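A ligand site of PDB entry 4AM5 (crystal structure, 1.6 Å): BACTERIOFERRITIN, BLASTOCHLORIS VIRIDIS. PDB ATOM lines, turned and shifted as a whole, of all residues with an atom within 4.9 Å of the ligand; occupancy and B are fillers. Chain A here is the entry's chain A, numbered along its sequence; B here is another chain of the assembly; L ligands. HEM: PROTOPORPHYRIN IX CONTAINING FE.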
ATOM      1  N   LEU A  19     -13.549  -4.462  11.608  1.00  0.00           N
ATOM      2  CA  LEU A  19     -14.932  -4.666  11.281  1.00  0.00           C
ATOM      3  C   LEU A  19     -15.795  -3.510  11.894  1.00  0.00           C
ATOM      4  O   LEU A  19     -16.832  -3.065  11.281  1.00  0.00           O
ATOM      5  CB  LEU A  19     -15.428  -5.976  11.906  1.00  0.00           C
ATOM      6  CG  LEU A  19     -14.754  -7.200  11.246  1.00  0.00           C
ATOM      7  CD1 LEU A  19     -15.068  -8.463  12.054  1.00  0.00           C
ATOM      8  CD2 LEU A  19     -15.289  -7.336   9.806  1.00  0.00           C
ATOM      9  N   VAL A  22     -15.272  -0.527   9.586  1.00  0.00           N
ATOM     10  CA  VAL A  22     -16.040  -0.646   8.327  1.00  0.00           C
ATOM     11  C   VAL A  22     -17.486  -0.203   8.565  1.00  0.00           C
ATOM     12  O   VAL A  22     -18.039   0.542   7.752  1.00  0.00           O
ATOM     13  CB  VAL A  22     -16.013  -2.169   7.882  1.00  0.00           C
ATOM     14  CG1 VAL A  22     -17.066  -2.403   6.734  1.00  0.00           C
ATOM     15  CG2 VAL A  22     -14.593  -2.534   7.324  1.00  0.00           C
ATOM     16  N   SER A  23     -18.156  -0.779   9.573  1.00  0.00           N
ATOM     17  CA  SER A  23     -19.579  -0.478   9.737  1.00  0.00           C
ATOM     18  C   SER A  23     -19.818   0.934  10.254  1.00  0.00           C
ATOM     19  O   SER A  23     -20.815   1.568   9.879  1.00  0.00           O
ATOM     20  CB  SER A  23     -20.166  -1.497  10.763  1.00  0.00           C
ATOM     21  OG  SER A  23     -20.413  -2.746  10.107  1.00  0.00           O
ATOM     22  N   TRP A  26     -19.368   3.048   7.266  1.00  0.00           N
ATOM     23  CA  TRP A  26     -20.413   2.913   6.243  1.00  0.00           C
ATOM     24  C   TRP A  26     -21.712   3.588   6.730  1.00  0.00           C
ATOM     25  O   TRP A  26     -22.447   4.226   5.961  1.00  0.00           O
ATOM     26  CB  TRP A  26     -20.666   1.389   6.000  1.00  0.00           C
ATOM     27  CG  TRP A  26     -21.431   1.187   4.720  1.00  0.00           C
ATOM     28  CD1 TRP A  26     -22.817   1.219   4.587  1.00  0.00           C
ATOM     29  CD2 TRP A  26     -20.884   1.196   3.403  1.00  0.00           C
ATOM     30  NE1 TRP A  26     -23.176   1.187   3.266  1.00  0.00           N
ATOM     31  CE2 TRP A  26     -22.033   1.201   2.476  1.00  0.00           C
ATOM     32  CE3 TRP A  26     -19.618   1.181   2.912  1.00  0.00           C
ATOM     33  CZ2 TRP A  26     -21.867   1.103   1.095  1.00  0.00           C
ATOM     34  CZ3 TRP A  26     -19.444   1.167   1.554  1.00  0.00           C
ATOM     35  CH2 TRP A  26     -20.522   1.120   0.649  1.00  0.00           C
ATOM     36  N   ARG A  45     -17.592   6.773   2.358  1.00  0.00           N
ATOM     37  CA  ARG A  45     -17.700   5.471   1.637  1.00  0.00           C
ATOM     38  C   ARG A  45     -16.279   4.935   1.301  1.00  0.00           C
ATOM     39  O   ARG A  45     -16.006   3.748   1.520  1.00  0.00           O
ATOM     40  CB  ARG A  45     -18.545   5.685   0.370  1.00  0.00           C
ATOM     41  CG  ARG A  45     -18.882   4.348  -0.310  1.00  0.00           C
ATOM     42  CD  ARG A  45     -19.751   4.696  -1.534  1.00  0.00           C
ATOM     43  NE  ARG A  45     -20.474   3.533  -2.052  1.00  0.00           N
ATOM     44  CZ  ARG A  45     -19.986   2.692  -2.902  1.00  0.00           C
ATOM     45  NH1 ARG A  45     -18.725   2.781  -3.226  1.00  0.00           N
ATOM     46  NH2 ARG A  45     -20.779   1.652  -3.325  1.00  0.00           N
ATOM     47  N   ILE A  49     -14.385   1.456   2.652  1.00  0.00           N
ATOM     48  CA  ILE A  49     -13.786   0.420   1.770  1.00  0.00           C
ATOM     49  C   ILE A  49     -12.305   0.232   2.049  1.00  0.00           C
ATOM     50  O   ILE A  49     -11.809  -0.935   1.935  1.00  0.00           O
ATOM     51  CB  ILE A  49     -14.136   0.860   0.319  1.00  0.00           C
ATOM     52  CG1 ILE A  49     -15.627   0.628   0.121  1.00  0.00           C
ATOM     53  CG2 ILE A  49     -13.429  -0.079  -0.676  1.00  0.00           C
ATOM     54  CD1 ILE A  49     -16.151   1.230  -1.172  1.00  0.00           C
ATOM     55  N   MET A  52     -12.273  -2.125   4.853  1.00  0.00           N
ATOM     56  CA  MET A  52     -12.649  -3.474   4.416  1.00  0.00           C
ATOM     57  C   MET A  52     -11.329  -4.184   3.971  1.00  0.00           C
ATOM     58  O   MET A  52     -11.168  -5.410   4.263  1.00  0.00           O
ATOM     59  CB  MET A  52     -13.658  -3.428   3.251  1.00  0.00           C
ATOM     60  CG  MET A  52     -15.053  -2.910   3.756  1.00  0.00           C
ATOM     61  SD  MET A  52     -16.108  -2.728   2.288  1.00  0.00           S
ATOM     62  CE  MET A  52     -17.251  -1.465   2.933  1.00  0.00           C
ATOM     63  N   ALA A  53     -10.421  -3.519   3.263  1.00  0.00           N
ATOM     64  CA  ALA A  53      -9.207  -4.139   2.872  1.00  0.00           C
ATOM     65  C   ALA A  53      -8.332  -4.558   4.058  1.00  0.00           C
ATOM     66  O   ALA A  53      -7.722  -5.608   4.057  1.00  0.00           O
ATOM     67  CB  ALA A  53      -8.436  -3.209   1.882  1.00  0.00           C
ATOM     68  N   ALA A  55      -9.497  -5.267   7.090  1.00  0.00           N
ATOM     69  CA  ALA A  55     -10.121  -6.452   7.726  1.00  0.00           C
ATOM     70  C   ALA A  55      -9.688  -7.713   6.968  1.00  0.00           C
ATOM     71  O   ALA A  55      -9.345  -8.730   7.610  1.00  0.00           O
ATOM     72  CB  ALA A  55     -11.638  -6.265   7.708  1.00  0.00           C
ATOM     73  N   ASP A  56      -9.731  -7.665   5.618  1.00  0.00           N
ATOM     74  CA  ASP A  56      -9.340  -8.824   4.866  1.00  0.00           C
ATOM     75  C   ASP A  56      -7.896  -9.215   5.116  1.00  0.00           C
ATOM     76  O   ASP A  56      -7.585 -10.408   5.177  1.00  0.00           O
ATOM     77  CB  ASP A  56      -9.585  -8.468   3.371  1.00  0.00           C
ATOM     78  CG  ASP A  56      -9.293  -9.631   2.463  1.00  0.00           C
ATOM     79  OD1 ASP A  56      -9.649 -10.745   2.737  1.00  0.00           O
ATOM     80  OD2 ASP A  56      -8.573  -9.413   1.456  1.00  0.00           O
ATOM     81  N   LEU A  71     -15.128 -13.137  13.272  1.00  0.00           N
ATOM     82  CA  LEU A  71     -15.842 -11.956  12.741  1.00  0.00           C
ATOM     83  C   LEU A  71     -17.190 -11.820  13.473  1.00  0.00           C
ATOM     84  O   LEU A  71     -18.042 -11.064  13.033  1.00  0.00           O
ATOM     85  CB  LEU A  71     -16.072 -12.167  11.245  1.00  0.00           C
ATOM     86  CG  LEU A  71     -14.784 -12.077  10.371  1.00  0.00           C
ATOM     87  CD1 LEU A  71     -14.087 -13.428  10.335  1.00  0.00           C
ATOM     88  CD2 LEU A  71     -15.167 -11.798   8.902  1.00  0.00           C
ATOM     89  N   LEU B  19     -25.501  -8.529   7.280  1.00  0.00           N
ATOM     90  CA  LEU B  19     -24.167  -8.407   7.829  1.00  0.00           C
ATOM     91  C   LEU B  19     -23.554  -9.779   8.187  1.00  0.00           C
ATOM     92  O   LEU B  19     -22.338 -10.018   8.071  1.00  0.00           O
ATOM     93  CB  LEU B  19     -24.140  -7.517   9.112  1.00  0.00           C
ATOM     94  CG  LEU B  19     -24.596  -6.052   8.798  1.00  0.00           C
ATOM     95  CD1 LEU B  19     -24.904  -5.345  10.132  1.00  0.00           C
ATOM     96  CD2 LEU B  19     -23.404  -5.351   8.041  1.00  0.00           C
ATOM     97  N   VAL B  22     -22.496 -11.377   4.886  1.00  0.00           N
ATOM     98  CA  VAL B  22     -21.286 -10.801   4.352  1.00  0.00           C
ATOM     99  C   VAL B  22     -20.077 -11.471   5.048  1.00  0.00           C
ATOM    100  O   VAL B  22     -19.107 -11.913   4.369  1.00  0.00           O
ATOM    101  CB  VAL B  22     -21.262  -9.286   4.696  1.00  0.00           C
ATOM    102  CG1 VAL B  22     -19.826  -8.763   4.400  1.00  0.00           C
ATOM    103  CG2 VAL B  22     -22.226  -8.505   3.778  1.00  0.00           C
ATOM    104  N   SER B  23     -20.087 -11.474   6.387  1.00  0.00           N
ATOM    105  CA  SER B  23     -18.906 -11.991   7.098  1.00  0.00           C
ATOM    106  C   SER B  23     -18.775 -13.515   6.976  1.00  0.00           C
ATOM    107  O   SER B  23     -17.646 -14.032   6.911  1.00  0.00           O
ATOM    108  CB  SER B  23     -18.965 -11.604   8.603  1.00  0.00           C
ATOM    109  OG  SER B  23     -18.625 -10.217   8.693  1.00  0.00           O
ATOM    110  N   TRP B  26     -17.444 -14.080   3.561  1.00  0.00           N
ATOM    111  CA  TRP B  26     -16.041 -13.625   3.360  1.00  0.00           C
ATOM    112  C   TRP B  26     -15.052 -14.577   4.099  1.00  0.00           C
ATOM    113  O   TRP B  26     -13.995 -14.918   3.559  1.00  0.00           O
ATOM    114  CB  TRP B  26     -15.880 -12.174   3.966  1.00  0.00           C
ATOM    115  CG  TRP B  26     -14.620 -11.560   3.463  1.00  0.00           C
ATOM    116  CD1 TRP B  26     -13.352 -11.706   4.026  1.00  0.00           C
ATOM    117  CD2 TRP B  26     -14.448 -10.880   2.201  1.00  0.00           C
ATOM    118  NE1 TRP B  26     -12.376 -11.129   3.186  1.00  0.00           N
ATOM    119  CE2 TRP B  26     -13.006 -10.583   2.054  1.00  0.00           C
ATOM    120  CE3 TRP B  26     -15.319 -10.510   1.222  1.00  0.00           C
ATOM    121  CZ2 TRP B  26     -12.526  -9.914   0.919  1.00  0.00           C
ATOM    122  CZ3 TRP B  26     -14.854  -9.909   0.089  1.00  0.00           C
ATOM    123  CH2 TRP B  26     -13.482  -9.582  -0.077  1.00  0.00           C
ATOM    124  N   ARG B  45     -16.157 -15.038  -2.632  1.00  0.00           N
ATOM    125  CA  ARG B  45     -15.829 -13.577  -2.520  1.00  0.00           C
ATOM    126  C   ARG B  45     -16.968 -12.767  -3.245  1.00  0.00           C
ATOM    127  O   ARG B  45     -17.456 -11.755  -2.729  1.00  0.00           O
ATOM    128  CB  ARG B  45     -14.487 -13.338  -3.199  1.00  0.00           C
ATOM    129  CG  ARG B  45     -14.003 -11.893  -2.972  1.00  0.00           C
ATOM    130  CD  ARG B  45     -12.638 -11.727  -3.707  1.00  0.00           C
ATOM    131  NE  ARG B  45     -11.873 -10.596  -3.142  1.00  0.00           N
ATOM    132  CZ  ARG B  45     -11.990  -9.400  -3.609  1.00  0.00           C
ATOM    133  NH1 ARG B  45     -12.874  -9.182  -4.569  1.00  0.00           N
ATOM    134  NH2 ARG B  45     -11.225  -8.377  -3.123  1.00  0.00           N
ATOM    135  N   ILE B  49     -19.721 -10.025  -1.638  1.00  0.00           N
ATOM    136  CA  ILE B  49     -19.919  -8.646  -2.166  1.00  0.00           C
ATOM    137  C   ILE B  49     -21.377  -8.407  -2.607  1.00  0.00           C
ATOM    138  O   ILE B  49     -21.907  -7.277  -2.406  1.00  0.00           O
ATOM    139  CB  ILE B  49     -18.843  -8.404  -3.287  1.00  0.00           C
ATOM    140  CG1 ILE B  49     -17.473  -8.320  -2.601  1.00  0.00           C
ATOM    141  CG2 ILE B  49     -19.128  -7.072  -3.964  1.00  0.00           C
ATOM    142  CD1 ILE B  49     -16.297  -8.353  -3.559  1.00  0.00           C
ATOM    143  N   MET B  52     -23.008  -7.504   0.560  1.00  0.00           N
ATOM    144  CA  MET B  52     -22.633  -6.142   1.000  1.00  0.00           C
ATOM    145  C   MET B  52     -23.636  -5.194   0.309  1.00  0.00           C
ATOM    146  O   MET B  52     -24.063  -4.260   0.995  1.00  0.00           O
ATOM    147  CB  MET B  52     -21.197  -5.819   0.549  1.00  0.00           C
ATOM    148  CG  MET B  52     -20.226  -6.671   1.390  1.00  0.00           C
ATOM    149  SD  MET B  52     -18.539  -6.349   0.729  1.00  0.00           S
ATOM    150  CE  MET B  52     -17.719  -7.908   1.218  1.00  0.00           C
ATOM    151  N   ALA B  55     -26.868  -5.372   2.261  1.00  0.00           N
ATOM    152  CA  ALA B  55     -26.776  -4.641   3.546  1.00  0.00           C
ATOM    153  C   ALA B  55     -26.944  -3.135   3.306  1.00  0.00           C
ATOM    154  O   ALA B  55     -27.687  -2.499   4.050  1.00  0.00           O
ATOM    155  CB  ALA B  55     -25.465  -4.935   4.219  1.00  0.00           C
ATOM    156  N   ASP B  56     -26.233  -2.631   2.285  1.00  0.00           N
ATOM    157  CA  ASP B  56     -26.369  -1.197   2.029  1.00  0.00           C
ATOM    158  C   ASP B  56     -27.793  -0.772   1.703  1.00  0.00           C
ATOM    159  O   ASP B  56     -28.232   0.275   2.150  1.00  0.00           O
ATOM    160  CB  ASP B  56     -25.393  -0.913   0.882  1.00  0.00           C
ATOM    161  CG  ASP B  56     -25.346   0.546   0.563  1.00  0.00           C
ATOM    162  OD1 ASP B  56     -25.306   1.431   1.419  1.00  0.00           O
ATOM    163  OD2 ASP B  56     -25.404   0.905  -0.647  1.00  0.00           O
ATOM    164  N   LEU B  71     -25.953  -1.711  13.087  1.00  0.00           N
ATOM    165  CA  LEU B  71     -24.913  -2.616  12.547  1.00  0.00           C
ATOM    166  C   LEU B  71     -24.090  -3.237  13.684  1.00  0.00           C
ATOM    167  O   LEU B  71     -23.055  -3.807  13.421  1.00  0.00           O
ATOM    168  CB  LEU B  71     -24.011  -1.780  11.637  1.00  0.00           C
ATOM    169  CG  LEU B  71     -24.713  -1.322  10.313  1.00  0.00           C
ATOM    170  CD1 LEU B  71     -25.496  -0.016  10.472  1.00  0.00           C
ATOM    171  CD2 LEU B  71     -23.587  -1.012   9.252  1.00  0.00           C
HETATM  172  CHA HEM L   1     -16.548  -3.860  -1.454  1.00  0.00           C
HETATM  173  CHB HEM L   1     -14.525  -6.498   1.981  1.00  0.00           C
HETATM  174  CHC HEM L   1     -18.253  -5.410   4.939  1.00  0.00           C
HETATM  175  CHD HEM L   1     -20.209  -2.679   1.319  1.00  0.00           C
HETATM  176  C1A HEM L   1     -15.593  -4.524  -0.751  1.00  0.00           C
HETATM  177  C2A HEM L   1     -14.298  -4.893  -1.239  1.00  0.00           C
HETATM  178  C3A HEM L   1     -13.693  -5.692  -0.237  1.00  0.00           C
HETATM  179  C4A HEM L   1     -14.703  -5.813   0.805  1.00  0.00           C
HETATM  180  CMA HEM L   1     -12.305  -6.265  -0.101  1.00  0.00           C
HETATM  181  CAA HEM L   1     -13.695  -4.323  -2.515  1.00  0.00           C
HETATM  182  CBA HEM L   1     -14.031  -5.473  -3.390  1.00  0.00           C
HETATM  183  CGA HEM L   1     -13.224  -5.316  -4.712  1.00  0.00           C
HETATM  184  O1A HEM L   1     -12.895  -6.353  -5.391  1.00  0.00           O
HETATM  185  O2A HEM L   1     -12.965  -4.095  -5.040  1.00  0.00           O
HETATM  186  C1B HEM L   1     -15.438  -6.486   3.082  1.00  0.00           C
HETATM  187  C2B HEM L   1     -15.208  -7.258   4.357  1.00  0.00           C
HETATM  188  C3B HEM L   1     -16.298  -6.931   5.118  1.00  0.00           C
HETATM  189  C4B HEM L   1     -17.103  -6.016   4.368  1.00  0.00           C
HETATM  190  CMB HEM L   1     -14.016  -8.183   4.616  1.00  0.00           C
HETATM  191  CAB HEM L   1     -16.722  -7.365   6.492  1.00  0.00           C
HETATM  192  CBB HEM L   1     -16.435  -8.657   6.486  1.00  0.00           C
HETATM  193  C1C HEM L   1     -19.071  -4.491   4.232  1.00  0.00           C
HETATM  194  C2C HEM L   1     -20.232  -3.856   4.830  1.00  0.00           C
HETATM  195  C3C HEM L   1     -20.818  -3.125   3.816  1.00  0.00           C
HETATM  196  C4C HEM L   1     -19.944  -3.272   2.603  1.00  0.00           C
HETATM  197  CMC HEM L   1     -20.641  -4.044   6.262  1.00  0.00           C
HETATM  198  CAC HEM L   1     -22.014  -2.242   3.794  1.00  0.00           C
HETATM  199  CBC HEM L   1     -22.928  -2.432   4.777  1.00  0.00           C
HETATM  200  C1D HEM L   1     -19.372  -2.806   0.191  1.00  0.00           C
HETATM  201  C2D HEM L   1     -19.726  -2.285  -1.090  1.00  0.00           C
HETATM  202  C3D HEM L   1     -18.620  -2.635  -1.866  1.00  0.00           C
HETATM  203  C4D HEM L   1     -17.776  -3.393  -1.006  1.00  0.00           C
HETATM  204  CMD HEM L   1     -20.982  -1.548  -1.398  1.00  0.00           C
HETATM  205  CAD HEM L   1     -18.383  -2.438  -3.389  1.00  0.00           C
HETATM  206  CBD HEM L   1     -18.029  -0.992  -3.469  1.00  0.00           C
HETATM  207  CGD HEM L   1     -17.960  -0.574  -4.945  1.00  0.00           C
HETATM  208  O1D HEM L   1     -17.923  -1.553  -5.788  1.00  0.00           O
HETATM  209  O2D HEM L   1     -17.887   0.691  -5.192  1.00  0.00           O
HETATM  210  NA  HEM L   1     -15.836  -5.052   0.499  1.00  0.00           N
HETATM  211  NB  HEM L   1     -16.566  -5.752   3.118  1.00  0.00           N
HETATM  212  NC  HEM L   1     -18.864  -4.104   2.861  1.00  0.00           N
HETATM  213  ND  HEM L   1     -18.185  -3.472   0.219  1.00  0.00           N
HETATM  214 FE   HEM L   1     -17.374  -4.592   1.712  1.00  0.00          FE
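O1A of the ligand lies within salt-bridge range of NH1 of Arg 45 of chain B. The side-chain sulfur of Met 52 of chain A is bound to an iron atom (FE) of the ligand (2.3 Å). The guanidinium group (NH1) of Arg 45 of chain A is in salt-bridge range of an oxygen (O2D) of the ligand (3.0 Å). An iron atom (FE) of the ligand is bound by the side-chain sulfur (SD) of Met 52 of chain B (2.3 Å).
Merely in contact with the ligand: Leu 19 of chain A (3.6 Å), Val 22 of chain A (3.7 Å), Trp 26 of chain A (3.4 Å), Ile 49 of chain A (3.7 Å), Leu 19 of chain B (3.5 Å), Val 22 of chain B (3.7 Å), Ser 23 of chain B (3.5 Å), Trp 26 of chain B (3.5 Å), Ile 49 of chain B (3.7 Å) and Ala 55 of chain B (3.6 Å). Hydrophobic or aromatic side chains within 4 Å of the ligand: Leu 19 of chain A, Val 22 of chain A, Trp 26 of chain A, Ile 49 of chain A, Met 52 of chain A, Leu 19 of chain B, Val 22 of chain B, Trp 26 of chain B, Ile 49 of chain B, Met 52 of chain B and Ala 55 of chain B. 14 residues have an atom within 4 Å of the ligand: Leu 19 of chain A, Val 22 of chain A, Trp 26 of chain A, Arg 45 of chain A, Ile 49 of chain A, Met 52 of chain A, Leu 19 of chain B, Val 22 of chain B, Ser 23 of chain B, Trp 26 of chain B, Arg 45 of chain B, Ile 49 of chain B, Met 52 of chain B and Ala 55 of chain B.
NE1 of Trp 26 of chain A is in hydrogen-bond range of OD1 of Asp 56 of chain B (2.8 Å). The indole nitrogen of Trp 26 of chain B sits at hydrogen-bond distance from the side-chain carboxylate of Asp 56 of chain A.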
